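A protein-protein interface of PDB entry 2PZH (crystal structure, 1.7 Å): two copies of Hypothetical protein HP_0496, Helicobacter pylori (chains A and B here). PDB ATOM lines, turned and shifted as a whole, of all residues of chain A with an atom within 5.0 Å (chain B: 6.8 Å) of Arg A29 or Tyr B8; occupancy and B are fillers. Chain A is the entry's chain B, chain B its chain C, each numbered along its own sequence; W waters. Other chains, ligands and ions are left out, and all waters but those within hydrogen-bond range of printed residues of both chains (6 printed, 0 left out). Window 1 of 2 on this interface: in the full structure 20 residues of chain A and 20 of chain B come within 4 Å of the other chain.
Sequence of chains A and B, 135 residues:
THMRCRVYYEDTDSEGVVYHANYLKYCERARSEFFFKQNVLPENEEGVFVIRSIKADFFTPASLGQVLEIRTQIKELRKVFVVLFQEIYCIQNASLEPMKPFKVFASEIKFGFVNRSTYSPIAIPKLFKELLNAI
OE2 of Glu B10 lies within salt-bridge range of NH2 of Arg A29 (2.8 Å). The guanidinium group of Arg B6 lies within salt-bridge range of the side-chain carboxylate of Glu A33 (2.8 Å). The side-chain carboxylate (OE2) of Glu A10 is in salt-bridge range of the guanidinium group (NH2) of Arg B29, 2.9 Å away. The side-chain hydroxyl (OH) of Tyr B8 lies within hydrogen-bond range of the side-chain carboxylate (OE1) of Glu A33, 2.9 Å away.
The backbone NH of Tyr B8 is in hydrogen-bond range of the side-chain carboxylate of Asp B11, at 2.9 Å. O of Val B7 sits at hydrogen-bond distance from N of Gly B65, at 2.8 Å. NH1 of Arg B6 lies within hydrogen-bond range of O of Gly B65, at 2.8 Å. The backbone NH (N) of Val B7 is in hydrogen-bond range of the backbone carbonyl oxygen (O) of Gln B66 (2.9 Å). O of Tyr B9 lies within hydrogen-bond range of OG1 of Thr B12 (2.8 Å). The side-chain hydroxyl of Ser A32 lies within hydrogen-bond range of the side-chain carboxylate of Glu A28 (2.5 Å).
Glu A10 touches Arg B29, and with the chains exchanged Arg A29 touches Glu B10. Of the 12 pairs that touch across the chains among the printed residues, 2 have their exchanged pair printed and touching as well.
Printed residues of chain A that touch a printed residue of chain B: Glu A10, Lys A25, Glu A28, Arg A29, Ser A32, Glu A33 and Phe A36. Along chain A the printed residues that touch a printed residue of chain B span positions 10 to 36. Printed residues of chain B that touch a printed residue of chain A: Arg B6, Val B7, Tyr B8, Tyr B9, Glu B10, Arg B29 and Gly B65. Hydrophobic or aromatic side chains of chain B within 4 Å of the printed part of chain A: Tyr B8 and Tyr B9. Among the printed residues, 12 pairs touch across the chains. Among the printed residues, Asp or Glu carboxylates within 4 Å of a Lys or Arg side-chain nitrogen of the other chain: Glu A10 with Arg B29 (2.9 Å), Arg A29 with Glu B10 (2.8 Å) and Glu A33 with Arg B6 (2.8 Å).
Of chain B, only Tyr B8 (3.5 Å) and Glu B10 (2.8 Å) come within 4 Å of Arg A29. Printed residues of chain B within 4 Å of Glu A33: Arg B6 (2.8 Å) and Tyr B8 (2.9 Å). Of the printed residues of chain A, Arg B6 touches Glu A33 (2.8 Å) and Phe A36 (3.5 Å). Printed residues of chain A within 4 Å of Tyr B9: Glu A28 and Ser A32. The nearest residue of chain B that does not touch Arg A29 is Arg B29 (4.3 Å). The nearest residue of chain A that does not touch Tyr B8 is Glu A28 (4.03 Å).
OE2 of Glu B10 touches CD of Lys A25, at 3.6 Å. CD1 of Tyr B9 touches OE1 of Glu A28 (3.6 Å). Tyr B8 touches Arg A29. Ser A32 touches Tyr B9. CD2 of Phe A36 touches CD of Arg B6, at 3.5 Å. Phe A36 touches Val B7. CD1 of Tyr B8 touches CE2 of Phe A36, at 3.6 Å. Phe A36 touches Gly B65 (CZ to CA, 3.6 Å).
Water W6 bridges the side-chain carboxylate of Glu A28 and the side-chain carboxylate of Glu B10. Water W5 lies within hydrogen-bond range of OE2 of Glu A28, N of Tyr B9 and OG of Ser A32. Water W3 lies within hydrogen-bond range of O of Phe A36 (2.8 Å) and NH2 of Arg B6 (3.1 Å). Water W2 bridges the backbone carbonyl oxygen (O) of Glu B10 and the side-chain amino group (NZ) of Lys A25. Water W4 bridges the side-chain carboxylate (OE2) of Glu B10 (2.9 Å) and the side-chain amino group (NZ) of Lys A25 (3.1 Å).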
ATOM      1  N   MET A   3      27.293  -5.553  18.520  1.00  0.00           N
ATOM      2  CA  MET A   3      26.071  -6.236  18.099  1.00  0.00           C
ATOM      3  C   MET A   3      25.575  -7.253  19.131  1.00  0.00           C
ATOM      4  O   MET A   3      26.373  -7.926  19.759  1.00  0.00           O
ATOM      5  CB  MET A   3      26.261  -6.907  16.745  1.00  0.00           C
ATOM      6  CG  MET A   3      24.950  -7.197  16.049  1.00  0.00           C
ATOM      7  SD  MET A   3      25.166  -8.219  14.594  1.00  0.00           S
ATOM      8  CE  MET A   3      25.456  -9.800  15.357  1.00  0.00           C
ATOM      9  N   CYS A   5      22.927 -10.590  20.064  1.00  0.00           N
ATOM     10  CA  CYS A   5      22.114 -11.653  19.505  1.00  0.00           C
ATOM     11  C   CYS A   5      21.725 -12.642  20.579  1.00  0.00           C
ATOM     12  O   CYS A   5      22.321 -12.720  21.638  1.00  0.00           O
ATOM     13  CB  CYS A   5      22.830 -12.360  18.365  1.00  0.00           C
ATOM     14  SG  CYS A   5      24.179 -13.350  18.941  1.00  0.00           S
ATOM     15  N   GLU A  10      18.535 -23.740  17.740  1.00  0.00           N
ATOM     16  CA  GLU A  10      19.373 -24.134  16.599  1.00  0.00           C
ATOM     17  C   GLU A  10      20.868 -24.013  16.912  1.00  0.00           C
ATOM     18  O   GLU A  10      21.708 -24.647  16.241  1.00  0.00           O
ATOM     19  CB  GLU A  10      19.055 -23.259  15.400  1.00  0.00           C
ATOM     20  CG  GLU A  10      19.521 -21.823  15.576  1.00  0.00           C
ATOM     21  CD  GLU A  10      18.894 -20.922  14.565  1.00  0.00           C
ATOM     22  OE1 GLU A  10      17.704 -20.568  14.742  1.00  0.00           O
ATOM     23  OE2 GLU A  10      19.572 -20.588  13.571  1.00  0.00           O
ATOM     24  N   ASP A  11      21.183 -23.168  17.898  1.00  0.00           N
ATOM     25  CA  ASP A  11      22.555 -22.828  18.295  1.00  0.00           C
ATOM     26  C   ASP A  11      23.188 -23.756  19.329  1.00  0.00           C
ATOM     27  O   ASP A  11      24.404 -23.767  19.473  1.00  0.00           O
ATOM     28  CB  ASP A  11      22.611 -21.405  18.879  1.00  0.00           C
ATOM     29  CG  ASP A  11      22.258 -20.342  17.867  1.00  0.00           C
ATOM     30  OD1 ASP A  11      22.560 -20.545  16.686  1.00  0.00           O
ATOM     31  OD2 ASP A  11      21.699 -19.286  18.260  1.00  0.00           O
ATOM     32  N   LYS A  25      29.933 -18.128  13.609  1.00  0.00           N
ATOM     33  CA  LYS A  25      28.785 -17.528  12.927  1.00  0.00           C
ATOM     34  C   LYS A  25      28.372 -16.177  13.532  1.00  0.00           C
ATOM     35  O   LYS A  25      28.130 -15.221  12.801  1.00  0.00           O
ATOM     36  CB  LYS A  25      27.586 -18.480  12.896  1.00  0.00           C
ATOM     37  CG  LYS A  25      27.857 -19.764  12.097  1.00  0.00           C
ATOM     38  CD  LYS A  25      26.582 -20.556  11.900  1.00  0.00           C
ATOM     39  CE  LYS A  25      26.863 -21.774  11.020  1.00  0.00           C
ATOM     40  NZ  LYS A  25      25.716 -22.730  10.839  1.00  0.00           N
ATOM     41  N   TYR A  26      28.244 -16.104  14.857  1.00  0.00           N
ATOM     42  CA  TYR A  26      27.932 -14.828  15.496  1.00  0.00           C
ATOM     43  C   TYR A  26      28.955 -13.756  15.120  1.00  0.00           C
ATOM     44  O   TYR A  26      28.608 -12.592  14.888  1.00  0.00           O
ATOM     45  CB  TYR A  26      27.938 -14.967  17.012  1.00  0.00           C
ATOM     46  CG  TYR A  26      26.912 -15.920  17.599  1.00  0.00           C
ATOM     47  CD1 TYR A  26      25.635 -16.055  17.048  1.00  0.00           C
ATOM     48  CD2 TYR A  26      27.217 -16.664  18.744  1.00  0.00           C
ATOM     49  CE1 TYR A  26      24.696 -16.917  17.618  1.00  0.00           C
ATOM     50  CE2 TYR A  26      26.286 -17.499  19.315  1.00  0.00           C
ATOM     51  CZ  TYR A  26      25.035 -17.635  18.742  1.00  0.00           C
ATOM     52  OH  TYR A  26      24.100 -18.482  19.329  1.00  0.00           O
ATOM     53  N   CYS A  27      30.224 -14.146  15.084  1.00  0.00           N
ATOM     54  CA  CYS A  27      31.281 -13.201  14.709  1.00  0.00           C
ATOM     55  C   CYS A  27      31.135 -12.761  13.262  1.00  0.00           C
ATOM     56  O   CYS A  27      31.308 -11.570  12.941  1.00  0.00           O
ATOM     57  CB  CYS A  27      32.678 -13.782  14.973  1.00  0.00           C
ATOM     58  SG  CYS A  27      33.076 -13.853  16.754  1.00  0.00           S
ATOM     59  N   GLU A  28      30.818 -13.706  12.379  1.00  0.00           N
ATOM     60  CA  GLU A  28      30.592 -13.352  10.985  1.00  0.00           C
ATOM     61  C   GLU A  28      29.426 -12.356  10.870  1.00  0.00           C
ATOM     62  O   GLU A  28      29.489 -11.374  10.121  1.00  0.00           O
ATOM     63  CB  GLU A  28      30.320 -14.608  10.139  1.00  0.00           C
ATOM     64  CG  GLU A  28      30.519 -14.416   8.609  1.00  0.00           C
ATOM     65  CD  GLU A  28      29.575 -13.403   7.981  1.00  0.00           C
ATOM     66  OE1 GLU A  28      30.063 -12.488   7.264  1.00  0.00           O
ATOM     67  OE2 GLU A  28      28.346 -13.523   8.174  1.00  0.00           O
ATOM     68  N   ARG A  29      28.338 -12.612  11.593  1.00  0.00           N
ATOM     69  CA  ARG A  29      27.194 -11.679  11.533  1.00  0.00           C
ATOM     70  C   ARG A  29      27.613 -10.260  11.918  1.00  0.00           C
ATOM     71  O   ARG A  29      27.185  -9.295  11.279  1.00  0.00           O
ATOM     72  CB  ARG A  29      26.058 -12.141  12.448  1.00  0.00           C
ATOM     73  CG  ARG A  29      25.483 -13.488  12.058  1.00  0.00           C
ATOM     74  CD  ARG A  29      24.429 -13.869  13.091  1.00  0.00           C
ATOM     75  NE  ARG A  29      24.211 -15.306  13.046  1.00  0.00           N
ATOM     76  CZ  ARG A  29      23.400 -15.966  13.864  1.00  0.00           C
ATOM     77  NH1 ARG A  29      22.737 -15.314  14.802  1.00  0.00           N
ATOM     78  NH2 ARG A  29      23.290 -17.291  13.746  1.00  0.00           N
ATOM     79  N   ALA A  30      28.419 -10.130  12.966  1.00  0.00           N
ATOM     80  CA  ALA A  30      28.833  -8.807  13.425  1.00  0.00           C
ATOM     81  C   ALA A  30      29.666  -8.104  12.352  1.00  0.00           C
ATOM     82  O   ALA A  30      29.509  -6.901  12.136  1.00  0.00           O
ATOM     83  CB  ALA A  30      29.605  -8.915  14.740  1.00  0.00           C
ATOM     84  N   ARG A  31      30.557  -8.849  11.689  1.00  0.00           N
ATOM     85  CA  ARG A  31      31.326  -8.290  10.564  1.00  0.00           C
ATOM     86  C   ARG A  31      30.416  -7.834   9.427  1.00  0.00           C
ATOM     87  O   ARG A  31      30.507  -6.699   8.953  1.00  0.00           O
ATOM     88  CB  ARG A  31      32.375  -9.287  10.037  1.00  0.00           C
ATOM     89  CG  ARG A  31      33.372  -9.718  11.103  1.00  0.00           C
ATOM     90  CD  ARG A  31      34.521 -10.493  10.497  1.00  0.00           C
ATOM     91  NE  ARG A  31      34.129 -11.768   9.899  1.00  0.00           N
ATOM     92  CZ  ARG A  31      34.093 -12.935  10.531  1.00  0.00           C
ATOM     93  NH1 ARG A  31      34.356 -13.010  11.831  1.00  0.00           N
ATOM     94  NH2 ARG A  31      33.757 -14.040   9.844  1.00  0.00           N
ATOM     95  N   SER A  32      29.541  -8.719   8.958  1.00  0.00           N
ATOM     96  CA  SER A  32      28.697  -8.369   7.833  1.00  0.00           C
ATOM     97  C   SER A  32      27.667  -7.284   8.128  1.00  0.00           C
ATOM     98  O   SER A  32      27.431  -6.393   7.297  1.00  0.00           O
ATOM     99  CB  SER A  32      28.071  -9.623   7.222  1.00  0.00           C
ATOM    100  OG  SER A  32      29.037 -10.319   6.438  1.00  0.00           O
ATOM    101  N   GLU A  33      27.078  -7.326   9.317  1.00  0.00           N
ATOM    102  CA  GLU A  33      26.086  -6.306   9.686  1.00  0.00           C
ATOM    103  C   GLU A  33      26.735  -4.907   9.684  1.00  0.00           C
ATOM    104  O   GLU A  33      26.073  -3.925   9.357  1.00  0.00           O
ATOM    105  CB  GLU A  33      25.425  -6.634  11.026  1.00  0.00           C
ATOM    106  CG  GLU A  33      24.219  -5.747  11.368  1.00  0.00           C
ATOM    107  CD  GLU A  33      23.082  -5.883  10.368  1.00  0.00           C
ATOM    108  OE1 GLU A  33      22.917  -6.987   9.779  1.00  0.00           O
ATOM    109  OE2 GLU A  33      22.341  -4.884  10.179  1.00  0.00           O
ATOM    110  N   PHE A  34      28.028  -4.824  10.005  1.00  0.00           N
ATOM    111  CA  PHE A  34      28.744  -3.545   9.960  1.00  0.00           C
ATOM    112  C   PHE A  34      28.581  -2.903   8.579  1.00  0.00           C
ATOM    113  O   PHE A  34      28.349  -1.699   8.449  1.00  0.00           O
ATOM    114  CB  PHE A  34      30.231  -3.746  10.292  1.00  0.00           C
ATOM    115  CG  PHE A  34      31.086  -2.530  10.031  1.00  0.00           C
ATOM    116  CD1 PHE A  34      31.091  -1.466  10.922  1.00  0.00           C
ATOM    117  CD2 PHE A  34      31.894  -2.462   8.901  1.00  0.00           C
ATOM    118  CE1 PHE A  34      31.892  -0.346  10.683  1.00  0.00           C
ATOM    119  CE2 PHE A  34      32.691  -1.347   8.655  1.00  0.00           C
ATOM    120  CZ  PHE A  34      32.686  -0.295   9.535  1.00  0.00           C
ATOM    121  N   PHE A  36      26.219  -4.078   6.161  1.00  0.00           N
ATOM    122  CA  PHE A  36      24.803  -4.032   5.819  1.00  0.00           C
ATOM    123  C   PHE A  36      24.135  -2.761   6.377  1.00  0.00           C
ATOM    124  O   PHE A  36      23.349  -2.112   5.691  1.00  0.00           O
ATOM    125  CB  PHE A  36      24.050  -5.242   6.392  1.00  0.00           C
ATOM    126  CG  PHE A  36      24.412  -6.567   5.790  1.00  0.00           C
ATOM    127  CD1 PHE A  36      24.937  -6.679   4.505  1.00  0.00           C
ATOM    128  CD2 PHE A  36      24.139  -7.727   6.504  1.00  0.00           C
ATOM    129  CE1 PHE A  36      25.241  -7.933   3.959  1.00  0.00           C
ATOM    130  CE2 PHE A  36      24.433  -8.972   5.983  1.00  0.00           C
ATOM    131  CZ  PHE A  36      24.984  -9.077   4.699  1.00  0.00           C
ATOM    132  N   CYS B   5      14.759 -10.739  10.692  1.00  0.00           N
ATOM    133  CA  CYS B   5      16.033 -11.463  10.573  1.00  0.00           C
ATOM    134  C   CYS B   5      16.759 -11.018   9.323  1.00  0.00           C
ATOM    135  O   CYS B   5      16.158 -10.868   8.275  1.00  0.00           O
ATOM    136  CB  CYS B   5      15.800 -12.970  10.472  1.00  0.00           C
ATOM    137  SG  CYS B   5      15.042 -13.702  11.927  1.00  0.00           S
ATOM    138  N   ARG B   6      18.070 -10.860   9.449  1.00  0.00           N
ATOM    139  CA  ARG B   6      18.938 -10.565   8.318  1.00  0.00           C
ATOM    140  C   ARG B   6      19.428 -11.861   7.680  1.00  0.00           C
ATOM    141  O   ARG B   6      19.739 -12.829   8.401  1.00  0.00           O
ATOM    142  CB  ARG B   6      20.163  -9.774   8.825  1.00  0.00           C
ATOM    143  CG  ARG B   6      21.178  -9.401   7.732  1.00  0.00           C
ATOM    144  CD  ARG B   6      20.686  -8.195   6.888  1.00  0.00           C
ATOM    145  NE  ARG B   6      20.795  -6.937   7.660  1.00  0.00           N
ATOM    146  CZ  ARG B   6      20.489  -5.724   7.203  1.00  0.00           C
ATOM    147  NH1 ARG B   6      20.071  -5.543   5.953  1.00  0.00           N
ATOM    148  NH2 ARG B   6      20.641  -4.664   8.003  1.00  0.00           N
ATOM    149  N   VAL B   7      19.567 -11.854   6.352  1.00  0.00           N
ATOM    150  CA  VAL B   7      20.178 -12.981   5.622  1.00  0.00           C
ATOM    151  C   VAL B   7      21.693 -12.803   5.604  1.00  0.00           C
ATOM    152  O   VAL B   7      22.217 -11.850   5.010  1.00  0.00           O
ATOM    153  CB  VAL B   7      19.610 -13.125   4.194  1.00  0.00           C
ATOM    154  CG1 VAL B   7      20.333 -14.242   3.414  1.00  0.00           C
ATOM    155  CG2 VAL B   7      18.096 -13.371   4.250  1.00  0.00           C
ATOM    156  N   TYR B   8      22.385 -13.711   6.295  1.00  0.00           N
ATOM    157  CA  TYR B   8      23.858 -13.726   6.343  1.00  0.00           C
ATOM    158  C   TYR B   8      24.433 -14.844   5.457  1.00  0.00           C
ATOM    159  O   TYR B   8      23.695 -15.706   4.942  1.00  0.00           O
ATOM    160  CB  TYR B   8      24.346 -13.881   7.791  1.00  0.00           C
ATOM    161  CG  TYR B   8      23.957 -12.734   8.697  1.00  0.00           C
ATOM    162  CD1 TYR B   8      24.592 -11.487   8.591  1.00  0.00           C
ATOM    163  CD2 TYR B   8      22.951 -12.889   9.662  1.00  0.00           C
ATOM    164  CE1 TYR B   8      24.224 -10.414   9.418  1.00  0.00           C
ATOM    165  CE2 TYR B   8      22.572 -11.818  10.484  1.00  0.00           C
ATOM    166  CZ  TYR B   8      23.223 -10.600  10.362  1.00  0.00           C
ATOM    167  OH  TYR B   8      22.856  -9.551  11.170  1.00  0.00           O
ATOM    168  N   TYR B   9      25.746 -14.835   5.265  1.00  0.00           N
ATOM    169  CA  TYR B   9      26.359 -15.835   4.387  1.00  0.00           C
ATOM    170  C   TYR B   9      26.035 -17.242   4.870  1.00  0.00           C
ATOM    171  O   TYR B   9      25.846 -18.158   4.059  1.00  0.00           O
ATOM    172  CB  TYR B   9      27.877 -15.655   4.335  1.00  0.00           C
ATOM    173  CG  TYR B   9      28.359 -14.525   3.453  1.00  0.00           C
ATOM    174  CD1 TYR B   9      28.976 -13.421   4.013  1.00  0.00           C
ATOM    175  CD2 TYR B   9      28.236 -14.577   2.061  1.00  0.00           C
ATOM    176  CE1 TYR B   9      29.440 -12.401   3.235  1.00  0.00           C
ATOM    177  CE2 TYR B   9      28.699 -13.539   1.269  1.00  0.00           C
ATOM    178  CZ  TYR B   9      29.303 -12.449   1.870  1.00  0.00           C
ATOM    179  OH  TYR B   9      29.789 -11.396   1.107  1.00  0.00           O
ATOM    180  N   GLU B  10      25.979 -17.413   6.188  1.00  0.00           N
ATOM    181  CA  GLU B  10      25.696 -18.725   6.788  1.00  0.00           C
ATOM    182  C   GLU B  10      24.347 -19.259   6.304  1.00  0.00           C
ATOM    183  O   GLU B  10      24.094 -20.477   6.347  1.00  0.00           O
ATOM    184  CB  GLU B  10      25.710 -18.637   8.311  1.00  0.00           C
ATOM    185  CG  GLU B  10      24.518 -17.919   8.882  1.00  0.00           C
ATOM    186  CD  GLU B  10      24.715 -17.521  10.319  1.00  0.00           C
ATOM    187  OE1 GLU B  10      25.512 -16.587  10.586  1.00  0.00           O
ATOM    188  OE2 GLU B  10      24.036 -18.117  11.191  1.00  0.00           O
ATOM    189  N   ASP B  11      23.483 -18.339   5.873  1.00  0.00           N
ATOM    190  CA  ASP B  11      22.100 -18.684   5.489  1.00  0.00           C
ATOM    191  C   ASP B  11      21.957 -19.021   4.030  1.00  0.00           C
ATOM    192  O   ASP B  11      20.945 -19.595   3.627  1.00  0.00           O
ATOM    193  CB  ASP B  11      21.161 -17.505   5.784  1.00  0.00           C
ATOM    194  CG  ASP B  11      21.117 -17.163   7.241  1.00  0.00           C
ATOM    195  OD1 ASP B  11      21.029 -18.101   8.040  1.00  0.00           O
ATOM    196  OD2 ASP B  11      21.157 -15.958   7.598  1.00  0.00           O
ATOM    197  N   THR B  12      22.935 -18.612   3.227  1.00  0.00           N
ATOM    198  CA  THR B  12      22.862 -18.752   1.772  1.00  0.00           C
ATOM    199  C   THR B  12      23.479 -20.065   1.307  1.00  0.00           C
ATOM    200  O   THR B  12      24.264 -20.680   2.033  1.00  0.00           O
ATOM    201  CB  THR B  12      23.627 -17.625   1.059  1.00  0.00           C
ATOM    202  OG1 THR B  12      25.011 -17.645   1.477  1.00  0.00           O
ATOM    203  CG2 THR B  12      22.979 -16.273   1.323  1.00  0.00           C
ATOM    204  N   VAL B  18      18.639 -18.277   0.101  1.00  0.00           N
ATOM    205  CA  VAL B  18      18.610 -18.931   1.395  1.00  0.00           C
ATOM    206  C   VAL B  18      18.407 -20.437   1.221  1.00  0.00           C
ATOM    207  O   VAL B  18      17.456 -20.884   0.546  1.00  0.00           O
ATOM    208  CB  VAL B  18      17.477 -18.339   2.290  1.00  0.00           C
ATOM    209  CG1 VAL B  18      17.279 -19.187   3.542  1.00  0.00           C
ATOM    210  CG2 VAL B  18      17.794 -16.857   2.622  1.00  0.00           C
ATOM    211  N   TYR B  26      14.403 -19.636  11.054  1.00  0.00           N
ATOM    212  CA  TYR B  26      13.813 -18.318  11.264  1.00  0.00           C
ATOM    213  C   TYR B  26      12.461 -18.415  11.980  1.00  0.00           C
ATOM    214  O   TYR B  26      12.204 -17.696  12.951  1.00  0.00           O
ATOM    215  CB  TYR B  26      13.635 -17.607   9.945  1.00  0.00           C
ATOM    216  CG  TYR B  26      14.908 -17.349   9.162  1.00  0.00           C
ATOM    217  CD1 TYR B  26      16.110 -17.069   9.799  1.00  0.00           C
ATOM    218  CD2 TYR B  26      14.874 -17.358   7.783  1.00  0.00           C
ATOM    219  CE1 TYR B  26      17.264 -16.799   9.058  1.00  0.00           C
ATOM    220  CE2 TYR B  26      16.006 -17.110   7.031  1.00  0.00           C
ATOM    221  CZ  TYR B  26      17.192 -16.826   7.667  1.00  0.00           C
ATOM    222  OH  TYR B  26      18.311 -16.566   6.889  1.00  0.00           O
ATOM    223  N   ARG B  29      13.035 -19.213  15.703  1.00  0.00           N
ATOM    224  CA  ARG B  29      13.477 -18.045  16.471  1.00  0.00           C
ATOM    225  C   ARG B  29      12.271 -17.209  16.873  1.00  0.00           C
ATOM    226  O   ARG B  29      12.169 -16.799  18.029  1.00  0.00           O
ATOM    227  CB  ARG B  29      14.449 -17.176  15.680  1.00  0.00           C
ATOM    228  CG  ARG B  29      15.735 -17.919  15.278  1.00  0.00           C
ATOM    229  CD  ARG B  29      16.577 -16.997  14.402  1.00  0.00           C
ATOM    230  NE  ARG B  29      17.620 -17.771  13.734  1.00  0.00           N
ATOM    231  CZ  ARG B  29      18.445 -17.242  12.832  1.00  0.00           C
ATOM    232  NH1 ARG B  29      18.336 -15.950  12.517  1.00  0.00           N
ATOM    233  NH2 ARG B  29      19.368 -18.008  12.235  1.00  0.00           N
ATOM    234  N   SER B  63      17.835 -13.464  -0.508  1.00  0.00           N
ATOM    235  CA  SER B  63      19.276 -13.503  -0.734  1.00  0.00           C
ATOM    236  C   SER B  63      20.035 -12.641   0.270  1.00  0.00           C
ATOM    237  O   SER B  63      19.432 -11.998   1.143  1.00  0.00           O
ATOM    238  CB  SER B  63      19.597 -13.023  -2.149  1.00  0.00           C
ATOM    239  OG  SER B  63      19.031 -11.745  -2.386  1.00  0.00           O
ATOM    240  N   LEU B  64      21.354 -12.653   0.117  1.00  0.00           N
ATOM    241  CA  LEU B  64      22.290 -12.045   1.038  1.00  0.00           C
ATOM    242  C   LEU B  64      21.915 -10.617   1.416  1.00  0.00           C
ATOM    243  O   LEU B  64      21.641  -9.791   0.542  1.00  0.00           O
ATOM    244  CB  LEU B  64      23.690 -12.072   0.413  1.00  0.00           C
ATOM    245  CG  LEU B  64      24.777 -11.534   1.341  1.00  0.00           C
ATOM    246  CD1 LEU B  64      24.964 -12.467   2.531  1.00  0.00           C
ATOM    247  CD2 LEU B  64      26.104 -11.300   0.595  1.00  0.00           C
ATOM    248  N   GLY B  65      21.873 -10.333   2.718  1.00  0.00           N
ATOM    249  CA  GLY B  65      21.744  -8.950   3.173  1.00  0.00           C
ATOM    250  C   GLY B  65      20.297  -8.501   3.290  1.00  0.00           C
ATOM    251  O   GLY B  65      20.021  -7.438   3.838  1.00  0.00           O
ATOM    252  N   GLN B  66      19.374  -9.298   2.770  1.00  0.00           N
ATOM    253  CA  GLN B  66      17.974  -8.902   2.818  1.00  0.00           C
ATOM    254  C   GLN B  66      17.452  -9.027   4.237  1.00  0.00           C
ATOM    255  O   GLN B  66      17.997  -9.788   5.048  1.00  0.00           O
ATOM    256  CB  GLN B  66      17.146  -9.689   1.804  1.00  0.00           C
ATOM    257  CG  GLN B  66      17.477  -9.328   0.359  1.00  0.00           C
ATOM    258  CD  GLN B  66      16.521  -9.926  -0.637  1.00  0.00           C
ATOM    259  OE1 GLN B  66      16.222 -11.119  -0.586  1.00  0.00           O
ATOM    260  NE2 GLN B  66      16.063  -9.111  -1.572  1.00  0.00           N
HETATM  261  O   HOH W   1      21.286 -18.635  15.095  1.00  0.00           O
HETATM  262  O   HOH W   2      25.569 -22.400   7.800  1.00  0.00           O
HETATM  263  O   HOH W   3      20.616  -2.046   6.365  1.00  0.00           O
HETATM  264  O   HOH W   4      23.284 -20.844  10.786  1.00  0.00           O
HETATM  265  O   HOH W   5      26.854 -12.360   6.127  1.00  0.00           O
HETATM  266  O   HOH W   6      27.267 -15.957   8.626  1.00  0.00           O
